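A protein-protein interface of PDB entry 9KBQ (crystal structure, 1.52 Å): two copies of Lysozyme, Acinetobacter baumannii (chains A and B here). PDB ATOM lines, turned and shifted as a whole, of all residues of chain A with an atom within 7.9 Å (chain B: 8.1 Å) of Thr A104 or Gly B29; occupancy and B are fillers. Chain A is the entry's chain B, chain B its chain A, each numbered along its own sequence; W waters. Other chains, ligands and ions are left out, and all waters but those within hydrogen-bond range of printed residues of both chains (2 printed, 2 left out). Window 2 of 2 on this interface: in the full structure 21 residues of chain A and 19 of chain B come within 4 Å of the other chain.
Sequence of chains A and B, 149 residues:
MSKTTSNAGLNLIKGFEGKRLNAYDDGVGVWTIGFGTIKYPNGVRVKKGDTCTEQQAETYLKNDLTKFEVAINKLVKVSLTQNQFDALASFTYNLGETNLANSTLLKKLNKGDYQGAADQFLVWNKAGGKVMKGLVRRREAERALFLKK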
ATOM      1  N   PHE A  91      17.815  17.574  -7.201  1.00  0.00           N
ATOM      2  CA  PHE A  91      17.780  16.134  -6.947  1.00  0.00           C
ATOM      3  C   PHE A  91      16.399  15.552  -7.241  1.00  0.00           C
ATOM      4  O   PHE A  91      16.270  14.519  -7.918  1.00  0.00           O
ATOM      5  CB  PHE A  91      18.192  15.912  -5.486  1.00  0.00           C
ATOM      6  CG  PHE A  91      18.164  14.480  -5.024  1.00  0.00           C
ATOM      7  CD1 PHE A  91      17.012  13.933  -4.476  1.00  0.00           C
ATOM      8  CD2 PHE A  91      19.317  13.713  -5.060  1.00  0.00           C
ATOM      9  CE1 PHE A  91      17.002  12.614  -4.022  1.00  0.00           C
ATOM     10  CE2 PHE A  91      19.318  12.403  -4.600  1.00  0.00           C
ATOM     11  CZ  PHE A  91      18.156  11.857  -4.083  1.00  0.00           C
ATOM     12  N   ASN A  99      11.377   8.722  -4.982  1.00  0.00           N
ATOM     13  CA  ASN A  99      12.756   8.469  -4.589  1.00  0.00           C
ATOM     14  C   ASN A  99      13.179   9.374  -3.436  1.00  0.00           C
ATOM     15  O   ASN A  99      13.855   8.917  -2.507  1.00  0.00           O
ATOM     16  CB  ASN A  99      13.689   8.631  -5.788  1.00  0.00           C
ATOM     17  CG  ASN A  99      13.737   7.381  -6.654  1.00  0.00           C
ATOM     18  OD1 ASN A  99      13.644   6.255  -6.149  1.00  0.00           O
ATOM     19  ND2 ASN A  99      13.881   7.571  -7.961  1.00  0.00           N
ATOM     20  N   LEU A 100      12.787  10.652  -3.467  1.00  0.00           N
ATOM     21  CA  LEU A 100      13.066  11.513  -2.319  1.00  0.00           C
ATOM     22  C   LEU A 100      12.370  10.995  -1.068  1.00  0.00           C
ATOM     23  O   LEU A 100      12.987  10.880  -0.001  1.00  0.00           O
ATOM     24  CB  LEU A 100      12.642  12.956  -2.605  1.00  0.00           C
ATOM     25  CG  LEU A 100      12.836  13.912  -1.415  1.00  0.00           C
ATOM     26  CD1 LEU A 100      14.311  14.115  -1.114  1.00  0.00           C
ATOM     27  CD2 LEU A 100      12.159  15.241  -1.689  1.00  0.00           C
ATOM     28  N   ALA A 101      11.083  10.657  -1.187  1.00  0.00           N
ATOM     29  CA  ALA A 101      10.298  10.242  -0.027  1.00  0.00           C
ATOM     30  C   ALA A 101      10.872   8.991   0.633  1.00  0.00           C
ATOM     31  O   ALA A 101      10.862   8.877   1.865  1.00  0.00           O
ATOM     32  CB  ALA A 101       8.840  10.015  -0.435  1.00  0.00           C
ATOM     33  N   ASN A 102      11.382   8.045  -0.157  1.00  0.00           N
ATOM     34  CA  ASN A 102      11.919   6.802   0.392  1.00  0.00           C
ATOM     35  C   ASN A 102      13.408   6.870   0.712  1.00  0.00           C
ATOM     36  O   ASN A 102      13.949   5.905   1.265  1.00  0.00           O
ATOM     37  CB  ASN A 102      11.692   5.635  -0.582  1.00  0.00           C
ATOM     38  CG  ASN A 102      10.229   5.393  -0.871  1.00  0.00           C
ATOM     39  OD1 ASN A 102       9.364   5.680  -0.042  1.00  0.00           O
ATOM     40  ND2 ASN A 102       9.943   4.846  -2.049  1.00  0.00           N
ATOM     41  N   SER A 103      14.076   7.975   0.391  1.00  0.00           N
ATOM     42  CA  SER A 103      15.531   8.007   0.422  1.00  0.00           C
ATOM     43  C   SER A 103      16.069   7.997   1.848  1.00  0.00           C
ATOM     44  O   SER A 103      15.471   8.565   2.768  1.00  0.00           O
ATOM     45  CB  SER A 103      16.059   9.249  -0.296  1.00  0.00           C
ATOM     46  OG  SER A 103      15.652  10.448   0.355  1.00  0.00           O
ATOM     47  N   THR A 104      17.228   7.351   2.010  1.00  0.00           N
ATOM     48  CA  THR A 104      18.006   7.509   3.239  1.00  0.00           C
ATOM     49  C   THR A 104      18.373   8.971   3.456  1.00  0.00           C
ATOM     50  O   THR A 104      18.444   9.439   4.601  1.00  0.00           O
ATOM     51  CB  THR A 104      19.270   6.653   3.173  1.00  0.00           C
ATOM     52  OG1 THR A 104      18.914   5.293   2.888  1.00  0.00           O
ATOM     53  CG2 THR A 104      20.034   6.705   4.496  1.00  0.00           C
ATOM     54  N   LEU A 105      18.620   9.702   2.364  1.00  0.00           N
ATOM     55  CA  LEU A 105      18.864  11.141   2.414  1.00  0.00           C
ATOM     56  C   LEU A 105      17.835  11.853   3.287  1.00  0.00           C
ATOM     57  O   LEU A 105      18.189  12.574   4.230  1.00  0.00           O
ATOM     58  CB  LEU A 105      18.850  11.707   0.981  1.00  0.00           C
ATOM     59  CG  LEU A 105      19.449  13.101   0.722  1.00  0.00           C
ATOM     60  CD1 LEU A 105      19.749  13.266  -0.767  1.00  0.00           C
ATOM     61  CD2 LEU A 105      18.536  14.229   1.205  1.00  0.00           C
ATOM     62  N   LEU A 106      16.550  11.659   2.974  1.00  0.00           N
ATOM     63  CA  LEU A 106      15.482  12.339   3.702  1.00  0.00           C
ATOM     64  C   LEU A 106      15.368  11.840   5.137  1.00  0.00           C
ATOM     65  O   LEU A 106      15.109  12.630   6.051  1.00  0.00           O
ATOM     66  CB  LEU A 106      14.154  12.157   2.972  1.00  0.00           C
ATOM     67  CG  LEU A 106      12.942  12.812   3.624  1.00  0.00           C
ATOM     68  CD1 LEU A 106      13.082  14.321   3.585  1.00  0.00           C
ATOM     69  CD2 LEU A 106      11.670  12.376   2.910  1.00  0.00           C
ATOM     70  N   LYS A 107      15.530  10.533   5.357  1.00  0.00           N
ATOM     71  CA  LYS A 107      15.514  10.004   6.720  1.00  0.00           C
ATOM     72  C   LYS A 107      16.558  10.707   7.587  1.00  0.00           C
ATOM     73  O   LYS A 107      16.254  11.228   8.676  1.00  0.00           O
ATOM     74  CB  LYS A 107      15.770   8.493   6.678  1.00  0.00           C
ATOM     75  CG  LYS A 107      15.384   7.736   7.934  1.00  0.00           C
ATOM     76  CD  LYS A 107      14.977   6.294   7.612  1.00  0.00           C
ATOM     77  CE  LYS A 107      14.069   6.212   6.390  1.00  0.00           C
ATOM     78  NZ  LYS A 107      14.004   4.830   5.833  1.00  0.00           N
ATOM     79  N   LYS A 108      17.798  10.759   7.095  1.00  0.00           N
ATOM     80  CA  LYS A 108      18.860  11.415   7.853  1.00  0.00           C
ATOM     81  C   LYS A 108      18.591  12.905   7.997  1.00  0.00           C
ATOM     82  O   LYS A 108      18.810  13.478   9.070  1.00  0.00           O
ATOM     83  CB  LYS A 108      20.210  11.177   7.181  1.00  0.00           C
ATOM     84  CG  LYS A 108      20.716   9.750   7.316  1.00  0.00           C
ATOM     85  CD  LYS A 108      22.132   9.610   6.809  1.00  0.00           C
ATOM     86  CE  LYS A 108      22.601   8.165   6.969  1.00  0.00           C
ATOM     87  NZ  LYS A 108      24.080   8.039   6.983  1.00  0.00           N
ATOM     88  N   LEU A 109      18.105  13.547   6.935  1.00  0.00           N
ATOM     89  CA  LEU A 109      17.822  14.977   6.995  1.00  0.00           C
ATOM     90  C   LEU A 109      16.805  15.286   8.088  1.00  0.00           C
ATOM     91  O   LEU A 109      16.990  16.214   8.888  1.00  0.00           O
ATOM     92  CB  LEU A 109      17.331  15.452   5.624  1.00  0.00           C
ATOM     93  CG  LEU A 109      16.962  16.927   5.481  1.00  0.00           C
ATOM     94  CD1 LEU A 109      18.099  17.782   6.005  1.00  0.00           C
ATOM     95  CD2 LEU A 109      16.652  17.261   4.029  1.00  0.00           C
ATOM     96  N   ASN A 110      15.726  14.508   8.151  1.00  0.00           N
ATOM     97  CA  ASN A 110      14.688  14.752   9.140  1.00  0.00           C
ATOM     98  C   ASN A 110      15.093  14.334  10.544  1.00  0.00           C
ATOM     99  O   ASN A 110      14.370  14.665  11.488  1.00  0.00           O
ATOM    100  CB  ASN A 110      13.387  14.064   8.725  1.00  0.00           C
ATOM    101  CG  ASN A 110      12.685  14.809   7.615  1.00  0.00           C
ATOM    102  OD1 ASN A 110      12.937  15.997   7.410  1.00  0.00           O
ATOM    103  ND2 ASN A 110      11.809  14.119   6.886  1.00  0.00           N
ATOM    104  N   LYS A 111      16.210  13.626  10.703  1.00  0.00           N
ATOM    105  CA  LYS A 111      16.792  13.458  12.032  1.00  0.00           C
ATOM    106  C   LYS A 111      17.687  14.623  12.439  1.00  0.00           C
ATOM    107  O   LYS A 111      18.239  14.604  13.546  1.00  0.00           O
ATOM    108  CB  LYS A 111      17.578  12.150  12.102  1.00  0.00           C
ATOM    109  CG  LYS A 111      16.688  10.923  12.051  1.00  0.00           C
ATOM    110  CD  LYS A 111      17.516   9.665  11.956  1.00  0.00           C
ATOM    111  CE  LYS A 111      16.635   8.434  12.033  1.00  0.00           C
ATOM    112  NZ  LYS A 111      17.454   7.200  12.147  1.00  0.00           N
ATOM    113  N   ASP A 113      20.414  15.356  10.706  1.00  0.00           N
ATOM    114  CA  ASP A 113      21.752  14.934  10.291  1.00  0.00           C
ATOM    115  C   ASP A 113      22.045  15.482   8.890  1.00  0.00           C
ATOM    116  O   ASP A 113      21.986  14.782   7.879  1.00  0.00           O
ATOM    117  CB  ASP A 113      21.851  13.412  10.343  1.00  0.00           C
ATOM    118  CG  ASP A 113      23.214  12.891   9.945  1.00  0.00           C
ATOM    119  OD1 ASP A 113      24.170  13.696   9.863  1.00  0.00           O
ATOM    120  OD2 ASP A 113      23.326  11.668   9.691  1.00  0.00           O
ATOM    121  N   GLY A 116      25.134  13.816   7.046  1.00  0.00           N
ATOM    122  CA  GLY A 116      24.774  12.514   6.506  1.00  0.00           C
ATOM    123  C   GLY A 116      23.867  12.628   5.295  1.00  0.00           C
ATOM    124  O   GLY A 116      24.047  11.915   4.298  1.00  0.00           O
ATOM    125  N   ALA A 117      22.890  13.539   5.360  1.00  0.00           N
ATOM    126  CA  ALA A 117      22.020  13.772   4.211  1.00  0.00           C
ATOM    127  C   ALA A 117      22.825  14.244   3.006  1.00  0.00           C
ATOM    128  O   ALA A 117      22.636  13.755   1.890  1.00  0.00           O
ATOM    129  CB  ALA A 117      20.932  14.788   4.573  1.00  0.00           C
ATOM    130  N   GLN A 120      24.471  11.469   1.340  1.00  0.00           N
ATOM    131  CA  GLN A 120      23.576  10.566   0.611  1.00  0.00           C
ATOM    132  C   GLN A 120      23.313  10.995  -0.832  1.00  0.00           C
ATOM    133  O   GLN A 120      22.896  10.157  -1.640  1.00  0.00           O
ATOM    134  CB  GLN A 120      22.245  10.402   1.344  1.00  0.00           C
ATOM    135  CG  GLN A 120      22.330   9.483   2.558  1.00  0.00           C
ATOM    136  CD  GLN A 120      22.647   8.059   2.161  1.00  0.00           C
ATOM    137  OE1 GLN A 120      21.931   7.455   1.365  1.00  0.00           O
ATOM    138  NE2 GLN A 120      23.713   7.506   2.731  1.00  0.00           N
ATOM    139  N   PHE A 121      23.491  12.278  -1.179  1.00  0.00           N
ATOM    140  CA  PHE A 121      23.351  12.669  -2.584  1.00  0.00           C
ATOM    141  C   PHE A 121      24.200  11.772  -3.478  1.00  0.00           C
ATOM    142  O   PHE A 121      23.752  11.334  -4.545  1.00  0.00           O
ATOM    143  CB  PHE A 121      23.759  14.136  -2.801  1.00  0.00           C
ATOM    144  CG  PHE A 121      22.720  15.160  -2.385  1.00  0.00           C
ATOM    145  CD1 PHE A 121      22.651  15.620  -1.074  1.00  0.00           C
ATOM    146  CD2 PHE A 121      21.843  15.692  -3.320  1.00  0.00           C
ATOM    147  CE1 PHE A 121      21.712  16.572  -0.703  1.00  0.00           C
ATOM    148  CE2 PHE A 121      20.903  16.646  -2.954  1.00  0.00           C
ATOM    149  CZ  PHE A 121      20.841  17.092  -1.642  1.00  0.00           C
ATOM    150  N   VAL A 123      25.025   8.743  -3.321  1.00  0.00           N
ATOM    151  CA  VAL A 123      24.613   7.353  -3.511  1.00  0.00           C
ATOM    152  C   VAL A 123      23.833   7.206  -4.814  1.00  0.00           C
ATOM    153  O   VAL A 123      23.841   6.137  -5.441  1.00  0.00           O
ATOM    154  CB  VAL A 123      23.790   6.876  -2.297  1.00  0.00           C
ATOM    155  CG1 VAL A 123      23.218   5.475  -2.528  1.00  0.00           C
ATOM    156  CG2 VAL A 123      24.627   6.914  -1.040  1.00  0.00           C
ATOM    157  N   TRP A 124      23.182   8.277  -5.262  1.00  0.00           N
ATOM    158  CA  TRP A 124      22.247   8.226  -6.386  1.00  0.00           C
ATOM    159  C   TRP A 124      22.964   8.539  -7.701  1.00  0.00           C
ATOM    160  O   TRP A 124      22.639   9.492  -8.414  1.00  0.00           O
ATOM    161  CB  TRP A 124      21.094   9.196  -6.153  1.00  0.00           C
ATOM    162  CG  TRP A 124      20.210   8.840  -5.002  1.00  0.00           C
ATOM    163  CD1 TRP A 124      20.422   9.130  -3.680  1.00  0.00           C
ATOM    164  CD2 TRP A 124      18.983   8.112  -5.062  1.00  0.00           C
ATOM    165  NE1 TRP A 124      19.386   8.646  -2.921  1.00  0.00           N
ATOM    166  CE2 TRP A 124      18.496   8.004  -3.746  1.00  0.00           C
ATOM    167  CE3 TRP A 124      18.246   7.534  -6.106  1.00  0.00           C
ATOM    168  CZ2 TRP A 124      17.296   7.366  -3.446  1.00  0.00           C
ATOM    169  CZ3 TRP A 124      17.063   6.893  -5.806  1.00  0.00           C
ATOM    170  CH2 TRP A 124      16.604   6.804  -4.487  1.00  0.00           C
ATOM    171  N   TYR B  24      25.654  -3.118  -3.272  1.00  0.00           N
ATOM    172  CA  TYR B  24      25.605  -1.662  -3.272  1.00  0.00           C
ATOM    173  C   TYR B  24      24.296  -1.183  -2.665  1.00  0.00           C
ATOM    174  O   TYR B  24      23.279  -1.879  -2.701  1.00  0.00           O
ATOM    175  CB  TYR B  24      25.766  -1.083  -4.690  1.00  0.00           C
ATOM    176  CG  TYR B  24      24.664  -1.458  -5.664  1.00  0.00           C
ATOM    177  CD1 TYR B  24      24.670  -2.692  -6.307  1.00  0.00           C
ATOM    178  CD2 TYR B  24      23.625  -0.582  -5.943  1.00  0.00           C
ATOM    179  CE1 TYR B  24      23.673  -3.042  -7.199  1.00  0.00           C
ATOM    180  CE2 TYR B  24      22.618  -0.925  -6.837  1.00  0.00           C
ATOM    181  CZ  TYR B  24      22.650  -2.155  -7.458  1.00  0.00           C
ATOM    182  OH  TYR B  24      21.657  -2.506  -8.346  1.00  0.00           O
ATOM    183  N   ASP B  25      24.344   0.021  -2.089  1.00  0.00           N
ATOM    184  CA  ASP B  25      23.154   0.717  -1.609  1.00  0.00           C
ATOM    185  C   ASP B  25      22.395   1.342  -2.771  1.00  0.00           C
ATOM    186  O   ASP B  25      22.977   2.077  -3.574  1.00  0.00           O
ATOM    187  CB  ASP B  25      23.540   1.817  -0.617  1.00  0.00           C
ATOM    188  CG  ASP B  25      22.377   2.262   0.262  1.00  0.00           C
ATOM    189  OD1 ASP B  25      21.216   2.135  -0.171  1.00  0.00           O
ATOM    190  OD2 ASP B  25      22.624   2.738   1.396  1.00  0.00           O
ATOM    191  N   ASP B  26      21.093   1.074  -2.846  1.00  0.00           N
ATOM    192  CA  ASP B  26      20.272   1.634  -3.915  1.00  0.00           C
ATOM    193  C   ASP B  26      19.755   3.033  -3.601  1.00  0.00           C
ATOM    194  O   ASP B  26      19.065   3.625  -4.442  1.00  0.00           O
ATOM    195  CB  ASP B  26      19.101   0.695  -4.240  1.00  0.00           C
ATOM    196  CG  ASP B  26      18.076   0.613  -3.127  1.00  0.00           C
ATOM    197  OD1 ASP B  26      18.302   1.183  -2.038  1.00  0.00           O
ATOM    198  OD2 ASP B  26      17.024  -0.028  -3.351  1.00  0.00           O
ATOM    199  N   GLY B  27      20.066   3.577  -2.425  1.00  0.00           N
ATOM    200  CA  GLY B  27      19.656   4.919  -2.060  1.00  0.00           C
ATOM    201  C   GLY B  27      18.502   4.973  -1.085  1.00  0.00           C
ATOM    202  O   GLY B  27      18.266   6.032  -0.479  1.00  0.00           O
ATOM    203  N   VAL B  28      17.757   3.883  -0.932  1.00  0.00           N
ATOM    204  CA  VAL B  28      16.715   3.786   0.078  1.00  0.00           C
ATOM    205  C   VAL B  28      17.136   2.836   1.198  1.00  0.00           C
ATOM    206  O   VAL B  28      16.306   2.390   1.989  1.00  0.00           O
ATOM    207  CB  VAL B  28      15.360   3.392  -0.537  1.00  0.00           C
ATOM    208  CG1 VAL B  28      14.990   4.342  -1.670  1.00  0.00           C
ATOM    209  CG2 VAL B  28      15.384   1.958  -1.049  1.00  0.00           C
ATOM    210  N   GLY B  29      18.428   2.540   1.278  1.00  0.00           N
ATOM    211  CA  GLY B  29      18.965   1.716   2.337  1.00  0.00           C
ATOM    212  C   GLY B  29      18.882   0.234   2.080  1.00  0.00           C
ATOM    213  O   GLY B  29      19.127  -0.553   3.000  1.00  0.00           O
ATOM    214  N   VAL B  30      18.558  -0.171   0.860  1.00  0.00           N
ATOM    215  CA  VAL B  30      18.366  -1.574   0.521  1.00  0.00           C
ATOM    216  C   VAL B  30      19.588  -2.029  -0.261  1.00  0.00           C
ATOM    217  O   VAL B  30      19.824  -1.591  -1.391  1.00  0.00           O
ATOM    218  CB  VAL B  30      17.074  -1.784  -0.276  1.00  0.00           C
ATOM    219  CG1 VAL B  30      16.969  -3.229  -0.756  1.00  0.00           C
ATOM    220  CG2 VAL B  30      15.874  -1.398   0.579  1.00  0.00           C
ATOM    221  N   TRP B  31      20.370  -2.924   0.329  1.00  0.00           N
ATOM    222  CA  TRP B  31      21.573  -3.390  -0.335  1.00  0.00           C
ATOM    223  C   TRP B  31      21.204  -4.395  -1.416  1.00  0.00           C
ATOM    224  O   TRP B  31      20.313  -5.229  -1.233  1.00  0.00           O
ATOM    225  CB  TRP B  31      22.545  -3.974   0.686  1.00  0.00           C
ATOM    226  CG  TRP B  31      23.146  -2.852   1.471  1.00  0.00           C
ATOM    227  CD1 TRP B  31      22.597  -2.226   2.552  1.00  0.00           C
ATOM    228  CD2 TRP B  31      24.375  -2.174   1.196  1.00  0.00           C
ATOM    229  NE1 TRP B  31      23.422  -1.216   2.984  1.00  0.00           N
ATOM    230  CE2 TRP B  31      24.520  -1.162   2.166  1.00  0.00           C
ATOM    231  CE3 TRP B  31      25.371  -2.329   0.229  1.00  0.00           C
ATOM    232  CZ2 TRP B  31      25.622  -0.314   2.198  1.00  0.00           C
ATOM    233  CZ3 TRP B  31      26.466  -1.486   0.264  1.00  0.00           C
ATOM    234  CH2 TRP B  31      26.581  -0.488   1.240  1.00  0.00           C
ATOM    235  N   THR B  32      21.873  -4.274  -2.560  1.00  0.00           N
ATOM    236  CA  THR B  32      21.461  -4.891  -3.811  1.00  0.00           C
ATOM    237  C   THR B  32      22.689  -5.498  -4.472  1.00  0.00           C
ATOM    238  O   THR B  32      23.796  -4.969  -4.337  1.00  0.00           O
ATOM    239  CB  THR B  32      20.807  -3.845  -4.730  1.00  0.00           C
ATOM    240  OG1 THR B  32      19.801  -3.133  -3.995  1.00  0.00           O
ATOM    241  CG2 THR B  32      20.159  -4.497  -5.942  1.00  0.00           C
ATOM    242  N   VAL B  46      20.441  -9.365   1.299  1.00  0.00           N
ATOM    243  CA  VAL B  46      21.738  -8.874   0.849  1.00  0.00           C
ATOM    244  C   VAL B  46      22.233  -7.807   1.818  1.00  0.00           C
ATOM    245  O   VAL B  46      21.449  -6.990   2.321  1.00  0.00           O
ATOM    246  CB  VAL B  46      21.612  -8.316  -0.580  1.00  0.00           C
ATOM    247  CG1 VAL B  46      22.911  -7.652  -1.035  1.00  0.00           C
ATOM    248  CG2 VAL B  46      21.174  -9.420  -1.557  1.00  0.00           C
ATOM    249  N   LYS B  47      23.537  -7.808   2.096  1.00  0.00           N
ATOM    250  CA  LYS B  47      24.107  -6.821   3.004  1.00  0.00           C
ATOM    251  C   LYS B  47      25.410  -6.270   2.442  1.00  0.00           C
ATOM    252  O   LYS B  47      26.022  -6.848   1.540  1.00  0.00           O
ATOM    253  CB  LYS B  47      24.343  -7.402   4.407  1.00  0.00           C
ATOM    254  CG  LYS B  47      25.363  -8.518   4.474  1.00  0.00           C
ATOM    255  CD  LYS B  47      25.300  -9.219   5.823  1.00  0.00           C
ATOM    256  CE  LYS B  47      26.493 -10.140   6.030  1.00  0.00           C
ATOM    257  NZ  LYS B  47      26.453 -11.314   5.116  1.00  0.00           N
HETATM  258  O   HOH W   1      23.256   3.593  -5.672  1.00  0.00           O
HETATM  259  O   HOH W   2      24.735   4.604   1.918  1.00  0.00           O
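The backbone carbonyl oxygen (O) of Gly B27 lies within hydrogen-bond range of the backbone NH (N) of Thr A104 (3.0 Å). The backbone NH (N) of Gly B29 lies within hydrogen-bond range of the side-chain hydroxyl (OG1) of Thr A104 (3.2 Å).
The backbone NH (N) of Gly B27 sits at hydrogen-bond distance from the side-chain carboxylate (OD1) of Asp B25 (2.9 Å). The side-chain carboxylate (OD1) of Asp B25 sits at hydrogen-bond distance from the backbone NH (N) of Gly B29, 3.2 Å away. N of Val B28 lies within hydrogen-bond range of OD1 of Asp B26, 3.0 Å away. OG of Ser A103 lies within hydrogen-bond range of O of Leu A100 (2.7 Å). N of Leu A106 lies within hydrogen-bond range of OG of Ser A103, 3.0 Å away.
Among the printed residues, pairs that only touch across the chains: Trp A124 with Gly B27 (3.4 Å), Asn A102 with Val B28 (3.4 Å), Thr A104 with Val B28 (3.5 Å), Ser A103 with Gly B27 (3.5 Å), Val A123 with Asp B25 (3.6 Å) and Val A123 with Gly B27 (3.6 Å).
Printed residues of chain B within 4 Å of Asn A102: Val B28. Of chain B, only Gly B27 (3.5 Å) comes within 4 Å of Ser A103. Printed residues of chain B within 4 Å of Val A123: Asp B25 (3.6 Å) and Gly B27 (3.6 Å). Of the printed residues of chain B, Trp A124 touches Gly B27. Printed residues of chain A within 4 Å of Asp B25: Val A123. Of the printed residues of chain A, Val B28 touches Asn A102 and Thr A104. Of chain A, only Thr A104 (3.2 Å) comes within 4 Å of Gly B29. The nearest residue of chain A that does not touch Gly B29 is Asn A102 (5.6 Å). The nearest printed residue of chain B that does not touch Trp A124 is Asp B26 (4.02 Å).
Hydrophobic or aromatic side chains of chain A within 4 Å of the printed part of chain B: Val A123 and Trp A124. Of the 11 printed residues of chain B, 4 touch a printed residue of chain A. Hydrophobic or aromatic side chains of chain B within 4 Å of the printed part of chain A: Val B28. Among the printed residues, 8 pairs touch across the chains. Among the printed residues, no Asp or Glu carboxylate lies within 4 Å of a Lys or Arg side-chain nitrogen of the other chain.
No position is printed for both chains. Of the 8 pairs that touch across the chains among the printed residues, none has its exchanged pair printed and touching as well.
Water W1 lies within hydrogen-bond range of O of Asp B25 (2.6 Å) and O of Val A123 (2.6 Å). Water W2 lies within hydrogen-bond range of OD2 of Asp B25 (2.9 Å) and NE2 of Gln A120 (3.2 Å).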
